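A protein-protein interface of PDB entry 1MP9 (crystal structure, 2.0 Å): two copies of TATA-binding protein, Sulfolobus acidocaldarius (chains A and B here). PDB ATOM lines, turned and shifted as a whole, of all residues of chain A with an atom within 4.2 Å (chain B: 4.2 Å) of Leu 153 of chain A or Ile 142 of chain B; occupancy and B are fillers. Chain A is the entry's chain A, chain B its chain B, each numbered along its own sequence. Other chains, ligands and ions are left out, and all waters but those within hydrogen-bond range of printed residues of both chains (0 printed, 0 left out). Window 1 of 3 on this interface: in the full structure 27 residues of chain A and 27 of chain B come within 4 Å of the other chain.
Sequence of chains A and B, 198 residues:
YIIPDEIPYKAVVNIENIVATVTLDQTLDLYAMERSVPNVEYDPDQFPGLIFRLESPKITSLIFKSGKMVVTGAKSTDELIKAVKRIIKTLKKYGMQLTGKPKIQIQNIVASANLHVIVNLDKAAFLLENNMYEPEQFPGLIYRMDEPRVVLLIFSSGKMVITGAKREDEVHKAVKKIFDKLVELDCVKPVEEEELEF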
ATOM      1  N   PHE A 138     -19.253   0.717 -26.066  1.00  0.00           N
ATOM      2  CA  PHE A 138     -19.372   2.006 -26.762  1.00  0.00           C
ATOM      3  C   PHE A 138     -19.162   1.613 -28.213  1.00  0.00           C
ATOM      4  O   PHE A 138     -18.221   0.905 -28.534  1.00  0.00           O
ATOM      5  CB  PHE A 138     -18.292   2.996 -26.281  1.00  0.00           C
ATOM      6  CG  PHE A 138     -18.253   4.278 -27.065  1.00  0.00           C
ATOM      7  CD1 PHE A 138     -19.233   5.240 -26.903  1.00  0.00           C
ATOM      8  CD2 PHE A 138     -17.234   4.516 -27.981  1.00  0.00           C
ATOM      9  CE1 PHE A 138     -19.201   6.422 -27.632  1.00  0.00           C
ATOM     10  CE2 PHE A 138     -17.200   5.693 -28.717  1.00  0.00           C
ATOM     11  CZ  PHE A 138     -18.185   6.647 -28.540  1.00  0.00           C
ATOM     12  N   LEU A 141     -14.438   3.892 -31.444  1.00  0.00           N
ATOM     13  CA  LEU A 141     -13.079   3.715 -30.943  1.00  0.00           C
ATOM     14  C   LEU A 141     -12.725   5.043 -30.260  1.00  0.00           C
ATOM     15  O   LEU A 141     -12.944   6.121 -30.830  1.00  0.00           O
ATOM     16  CB  LEU A 141     -12.113   3.460 -32.110  1.00  0.00           C
ATOM     17  CG  LEU A 141     -10.636   3.173 -31.730  1.00  0.00           C
ATOM     18  CD1 LEU A 141      -9.997   2.248 -32.751  1.00  0.00           C
ATOM     19  CD2 LEU A 141      -9.849   4.447 -31.630  1.00  0.00           C
ATOM     20  N   ILE A 142     -12.203   4.984 -29.047  1.00  0.00           N
ATOM     21  CA  ILE A 142     -11.848   6.204 -28.358  1.00  0.00           C
ATOM     22  C   ILE A 142     -10.333   6.277 -28.367  1.00  0.00           C
ATOM     23  O   ILE A 142      -9.645   5.329 -27.983  1.00  0.00           O
ATOM     24  CB  ILE A 142     -12.388   6.207 -26.896  1.00  0.00           C
ATOM     25  CG1 ILE A 142     -13.912   6.104 -26.926  1.00  0.00           C
ATOM     26  CG2 ILE A 142     -11.945   7.493 -26.158  1.00  0.00           C
ATOM     27  CD1 ILE A 142     -14.569   6.002 -25.540  1.00  0.00           C
ATOM     28  N   LEU A 152     -10.619  11.649 -29.055  1.00  0.00           N
ATOM     29  CA  LEU A 152     -11.367  11.425 -30.274  1.00  0.00           C
ATOM     30  C   LEU A 152     -12.333  10.265 -30.152  1.00  0.00           C
ATOM     31  O   LEU A 152     -11.983   9.245 -29.583  1.00  0.00           O
ATOM     32  CB  LEU A 152     -10.420  11.072 -31.409  1.00  0.00           C
ATOM     33  CG  LEU A 152      -9.234  11.987 -31.693  1.00  0.00           C
ATOM     34  CD1 LEU A 152      -8.424  11.410 -32.888  1.00  0.00           C
ATOM     35  CD2 LEU A 152      -9.763  13.405 -31.987  1.00  0.00           C
ATOM     36  N   LEU A 153     -13.541  10.423 -30.695  1.00  0.00           N
ATOM     37  CA  LEU A 153     -14.523   9.316 -30.751  1.00  0.00           C
ATOM     38  C   LEU A 153     -14.533   9.086 -32.271  1.00  0.00           C
ATOM     39  O   LEU A 153     -14.773  10.016 -33.022  1.00  0.00           O
ATOM     40  CB  LEU A 153     -15.907   9.755 -30.274  1.00  0.00           C
ATOM     41  CG  LEU A 153     -15.946  10.359 -28.873  1.00  0.00           C
ATOM     42  CD1 LEU A 153     -17.386  10.687 -28.508  1.00  0.00           C
ATOM     43  CD2 LEU A 153     -15.390   9.367 -27.847  1.00  0.00           C
ATOM     44  N   ILE A 154     -14.255   7.872 -32.717  1.00  0.00           N
ATOM     45  CA  ILE A 154     -14.166   7.564 -34.158  1.00  0.00           C
ATOM     46  C   ILE A 154     -15.112   6.417 -34.474  1.00  0.00           C
ATOM     47  O   ILE A 154     -15.008   5.333 -33.902  1.00  0.00           O
ATOM     48  CB  ILE A 154     -12.721   7.115 -34.513  1.00  0.00           C
ATOM     49  CG1 ILE A 154     -11.729   8.233 -34.139  1.00  0.00           C
ATOM     50  CG2 ILE A 154     -12.607   6.737 -36.034  1.00  0.00           C
ATOM     51  CD1 ILE A 154     -10.266   7.695 -34.164  1.00  0.00           C
ATOM     52  N   PHE A 155     -16.029   6.657 -35.395  1.00  0.00           N
ATOM     53  CA  PHE A 155     -17.009   5.646 -35.735  1.00  0.00           C
ATOM     54  C   PHE A 155     -16.693   5.027 -37.074  1.00  0.00           C
ATOM     55  O   PHE A 155     -16.025   5.639 -37.939  1.00  0.00           O
ATOM     56  CB  PHE A 155     -18.410   6.261 -35.723  1.00  0.00           C
ATOM     57  CG  PHE A 155     -18.787   6.888 -34.396  1.00  0.00           C
ATOM     58  CD1 PHE A 155     -18.619   8.252 -34.182  1.00  0.00           C
ATOM     59  CD2 PHE A 155     -19.319   6.108 -33.365  1.00  0.00           C
ATOM     60  CE1 PHE A 155     -18.971   8.843 -32.959  1.00  0.00           C
ATOM     61  CE2 PHE A 155     -19.676   6.691 -32.127  1.00  0.00           C
ATOM     62  CZ  PHE A 155     -19.494   8.069 -31.936  1.00  0.00           C
ATOM     63  N   LYS A 159     -17.457   9.148 -39.172  1.00  0.00           N
ATOM     64  CA  LYS A 159     -17.851  10.262 -38.335  1.00  0.00           C
ATOM     65  C   LYS A 159     -16.945  10.269 -37.120  1.00  0.00           C
ATOM     66  O   LYS A 159     -16.477   9.237 -36.672  1.00  0.00           O
ATOM     67  CB  LYS A 159     -19.281  10.120 -37.876  1.00  0.00           C
ATOM     68  CG  LYS A 159     -19.722  11.203 -36.888  1.00  0.00           C
ATOM     69  CD  LYS A 159     -21.209  11.069 -36.575  1.00  0.00           C
ATOM     70  CE  LYS A 159     -21.529   9.856 -35.678  1.00  0.00           C
ATOM     71  NZ  LYS A 159     -23.011   9.608 -35.553  1.00  0.00           N
ATOM     72  N   MET A 160     -16.704  11.452 -36.588  1.00  0.00           N
ATOM     73  CA  MET A 160     -15.815  11.577 -35.445  1.00  0.00           C
ATOM     74  C   MET A 160     -16.273  12.720 -34.596  1.00  0.00           C
ATOM     75  O   MET A 160     -16.910  13.669 -35.088  1.00  0.00           O
ATOM     76  CB  MET A 160     -14.396  11.972 -35.877  1.00  0.00           C
ATOM     77  CG  MET A 160     -13.474  10.949 -36.455  1.00  0.00           C
ATOM     78  SD  MET A 160     -12.016  11.916 -37.082  1.00  0.00           S
ATOM     79  CE  MET A 160     -11.274  12.470 -35.530  1.00  0.00           C
ATOM     80  N   VAL A 161     -15.900  12.649 -33.326  1.00  0.00           N
ATOM     81  CA  VAL A 161     -16.166  13.729 -32.411  1.00  0.00           C
ATOM     82  C   VAL A 161     -14.768  14.088 -31.845  1.00  0.00           C
ATOM     83  O   VAL A 161     -13.961  13.199 -31.504  1.00  0.00           O
ATOM     84  CB  VAL A 161     -17.086  13.299 -31.282  1.00  0.00           C
ATOM     85  CG1 VAL A 161     -17.225  14.440 -30.256  1.00  0.00           C
ATOM     86  CG2 VAL A 161     -18.470  12.945 -31.830  1.00  0.00           C
ATOM     87  N   ASN B 130     -12.103  19.425 -17.412  1.00  0.00           N
ATOM     88  CA  ASN B 130     -11.705  18.366 -18.338  1.00  0.00           C
ATOM     89  C   ASN B 130     -12.814  17.481 -18.886  1.00  0.00           C
ATOM     90  O   ASN B 130     -12.654  16.241 -18.927  1.00  0.00           O
ATOM     91  CB  ASN B 130     -10.689  17.466 -17.623  1.00  0.00           C
ATOM     92  CG  ASN B 130      -9.829  18.230 -16.621  1.00  0.00           C
ATOM     93  OD1 ASN B 130      -8.975  19.028 -17.000  1.00  0.00           O
ATOM     94  ND2 ASN B 130     -10.067  17.992 -15.325  1.00  0.00           N
ATOM     95  N   ASN B 131     -13.907  18.070 -19.356  1.00  0.00           N
ATOM     96  CA  ASN B 131     -14.972  17.217 -19.837  1.00  0.00           C
ATOM     97  C   ASN B 131     -15.761  17.742 -21.005  1.00  0.00           C
ATOM     98  O   ASN B 131     -15.740  18.925 -21.340  1.00  0.00           O
ATOM     99  CB  ASN B 131     -15.945  16.959 -18.692  1.00  0.00           C
ATOM    100  CG  ASN B 131     -16.952  18.082 -18.542  1.00  0.00           C
ATOM    101  OD1 ASN B 131     -17.926  18.150 -19.295  1.00  0.00           O
ATOM    102  ND2 ASN B 131     -16.708  18.995 -17.585  1.00  0.00           N
ATOM    103  N   MET B 132     -16.487  16.821 -21.615  1.00  0.00           N
ATOM    104  CA  MET B 132     -17.377  17.125 -22.707  1.00  0.00           C
ATOM    105  C   MET B 132     -18.760  16.559 -22.344  1.00  0.00           C
ATOM    106  O   MET B 132     -18.888  15.422 -21.859  1.00  0.00           O
ATOM    107  CB  MET B 132     -16.928  16.437 -24.002  1.00  0.00           C
ATOM    108  CG  MET B 132     -17.975  16.553 -25.138  1.00  0.00           C
ATOM    109  SD  MET B 132     -17.483  15.584 -26.587  1.00  0.00           S
ATOM    110  CE  MET B 132     -18.357  14.122 -26.322  1.00  0.00           C
ATOM    111  N   PHE B 138     -22.843  12.849 -28.109  1.00  0.00           N
ATOM    112  CA  PHE B 138     -22.683  11.628 -27.299  1.00  0.00           C
ATOM    113  C   PHE B 138     -23.565  11.831 -26.075  1.00  0.00           C
ATOM    114  O   PHE B 138     -23.454  12.842 -25.394  1.00  0.00           O
ATOM    115  CB  PHE B 138     -21.222  11.435 -26.875  1.00  0.00           C
ATOM    116  CG  PHE B 138     -21.036  10.298 -25.913  1.00  0.00           C
ATOM    117  CD1 PHE B 138     -21.391   9.003 -26.282  1.00  0.00           C
ATOM    118  CD2 PHE B 138     -20.539  10.520 -24.629  1.00  0.00           C
ATOM    119  CE1 PHE B 138     -21.255   7.942 -25.381  1.00  0.00           C
ATOM    120  CE2 PHE B 138     -20.399   9.457 -23.722  1.00  0.00           C
ATOM    121  CZ  PHE B 138     -20.759   8.168 -24.106  1.00  0.00           C
ATOM    122  N   GLY B 140     -23.495  10.629 -23.050  1.00  0.00           N
ATOM    123  CA  GLY B 140     -22.893  10.691 -21.734  1.00  0.00           C
ATOM    124  C   GLY B 140     -21.906  11.838 -21.573  1.00  0.00           C
ATOM    125  O   GLY B 140     -21.673  12.615 -22.500  1.00  0.00           O
ATOM    126  N   LEU B 141     -21.337  11.944 -20.381  1.00  0.00           N
ATOM    127  CA  LEU B 141     -20.345  12.969 -20.102  1.00  0.00           C
ATOM    128  C   LEU B 141     -19.002  12.250 -20.216  1.00  0.00           C
ATOM    129  O   LEU B 141     -18.835  11.131 -19.698  1.00  0.00           O
ATOM    130  CB  LEU B 141     -20.524  13.528 -18.677  1.00  0.00           C
ATOM    131  CG  LEU B 141     -19.469  14.612 -18.302  1.00  0.00           C
ATOM    132  CD1 LEU B 141     -20.072  15.605 -17.316  1.00  0.00           C
ATOM    133  CD2 LEU B 141     -18.231  13.957 -17.702  1.00  0.00           C
ATOM    134  N   ILE B 142     -18.048  12.866 -20.902  1.00  0.00           N
ATOM    135  CA  ILE B 142     -16.733  12.244 -21.050  1.00  0.00           C
ATOM    136  C   ILE B 142     -15.784  13.042 -20.184  1.00  0.00           C
ATOM    137  O   ILE B 142     -15.725  14.264 -20.310  1.00  0.00           O
ATOM    138  CB  ILE B 142     -16.228  12.309 -22.520  1.00  0.00           C
ATOM    139  CG1 ILE B 142     -17.120  11.444 -23.412  1.00  0.00           C
ATOM    140  CG2 ILE B 142     -14.766  11.798 -22.623  1.00  0.00           C
ATOM    141  CD1 ILE B 142     -16.679  11.478 -24.904  1.00  0.00           C
ATOM    142  N   TYR B 143     -15.043  12.349 -19.328  1.00  0.00           N
ATOM    143  CA  TYR B 143     -14.096  12.982 -18.406  1.00  0.00           C
ATOM    144  C   TYR B 143     -12.682  12.440 -18.627  1.00  0.00           C
ATOM    145  O   TYR B 143     -12.441  11.234 -18.551  1.00  0.00           O
ATOM    146  CB  TYR B 143     -14.503  12.709 -16.947  1.00  0.00           C
ATOM    147  CG  TYR B 143     -13.663  13.445 -15.907  1.00  0.00           C
ATOM    148  CD1 TYR B 143     -13.920  14.776 -15.609  1.00  0.00           C
ATOM    149  CD2 TYR B 143     -12.581  12.820 -15.261  1.00  0.00           C
ATOM    150  CE1 TYR B 143     -13.136  15.480 -14.710  1.00  0.00           C
ATOM    151  CE2 TYR B 143     -11.768  13.525 -14.341  1.00  0.00           C
ATOM    152  CZ  TYR B 143     -12.059  14.863 -14.075  1.00  0.00           C
ATOM    153  OH  TYR B 143     -11.313  15.611 -13.187  1.00  0.00           O
ATOM    154  N   VAL B 151      -9.941   7.538 -19.169  1.00  0.00           N
ATOM    155  CA  VAL B 151     -11.020   8.319 -19.747  1.00  0.00           C
ATOM    156  C   VAL B 151     -12.294   7.687 -19.198  1.00  0.00           C
ATOM    157  O   VAL B 151     -12.430   6.466 -19.176  1.00  0.00           O
ATOM    158  CB  VAL B 151     -11.003   8.283 -21.294  1.00  0.00           C
ATOM    159  CG1 VAL B 151     -12.291   8.913 -21.859  1.00  0.00           C
ATOM    160  CG2 VAL B 151      -9.780   9.079 -21.806  1.00  0.00           C
ATOM    161  N   LEU B 152     -13.204   8.531 -18.726  1.00  0.00           N
ATOM    162  CA  LEU B 152     -14.456   8.061 -18.174  1.00  0.00           C
ATOM    163  C   LEU B 152     -15.619   8.457 -19.071  1.00  0.00           C
ATOM    164  O   LEU B 152     -15.630   9.561 -19.584  1.00  0.00           O
ATOM    165  CB  LEU B 152     -14.703   8.709 -16.811  1.00  0.00           C
ATOM    166  CG  LEU B 152     -13.578   8.570 -15.777  1.00  0.00           C
ATOM    167  CD1 LEU B 152     -13.996   9.266 -14.438  1.00  0.00           C
ATOM    168  CD2 LEU B 152     -13.319   7.091 -15.571  1.00  0.00           C
ATOM    169  N   LEU B 153     -16.572   7.549 -19.255  1.00  0.00           N
ATOM    170  CA  LEU B 153     -17.827   7.852 -19.971  1.00  0.00           C
ATOM    171  C   LEU B 153     -18.814   7.739 -18.794  1.00  0.00           C
ATOM    172  O   LEU B 153     -18.847   6.714 -18.120  1.00  0.00           O
ATOM    173  CB  LEU B 153     -18.195   6.783 -21.015  1.00  0.00           C
ATOM    174  CG  LEU B 153     -17.180   6.574 -22.147  1.00  0.00           C
ATOM    175  CD1 LEU B 153     -17.803   5.684 -23.208  1.00  0.00           C
ATOM    176  CD2 LEU B 153     -16.801   7.900 -22.791  1.00  0.00           C
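O of Leu 153 of chain A is in hydrogen-bond range of N of Val 161 of chain A, 2.9 Å away.
N of Ile 142 of chain B is in hydrogen-bond range of O of Met 132 of chain B (2.9 Å).
Among the printed residues, pairs that only touch across the chains: Phe 138 of chain A with Phe 138 of chain B, Phe 138 of chain A with Leu 153 of chain B, Ile 142 of chain A with Leu 153 of chain B, Leu 153 of chain A with Ile 142 of chain B and Val 161 of chain A with Met 132 of chain B.
Of chain B, only Ile 142 (3.8 Å) comes within 4 Å of Leu 153 of chain A.
Ile 142 of chain B touches just one residue of chain A: Leu 153 (3.8 Å).
Of the printed residues of chain B, Ile 142 of chain A touches Leu 153 (3.9998 Å).
Of the printed residues of chain A, Met 132 of chain B touches Val 161.
Printed residues of chain B within 4 Å of Phe 138 of chain A: Phe 138 (3.4 Å) and Leu 153 (3.99 Å).
Of the printed residues of chain A, Leu 153 of chain B touches Phe 138 (3.99 Å) and Ile 142 (3.9998 Å).
Printed residues of chain A within 4 Å of Phe 138 of chain B: Phe 138.
Asn 130 of chain B touches none of the printed residues of chain A.
The nearest printed residue of chain B that does not touch Leu 153 of chain A is Met 132 of chain B (4.2 Å).
The nearest printed residue of chain B that does not touch Val 161 of chain A is Phe 138 of chain B (5.7 Å).
Hydrophobic or aromatic side chains of chain A that line the printed part of chain B: Phe 138, Ile 142, Leu 153 and Val 161.
Among the printed residues, 5 pairs touch across the chains.
Phe 138 of chain B touches its own counterpart, Phe 138 of chain A.
Phe 138 of chain A touches Leu 153 of chain B, but with the chains exchanged Leu 153 of chain A does not touch Phe 138 of chain B (4.2 Å).
Ile 142 of chain A touches Leu 153 of chain B, and with the chains exchanged Leu 153 of chain A touches Ile 142 of chain B.
5 positions are printed for both chains.
Of the 5 pairs that touch across the chains among the printed residues, 3 have their exchanged pair printed and touching as well.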
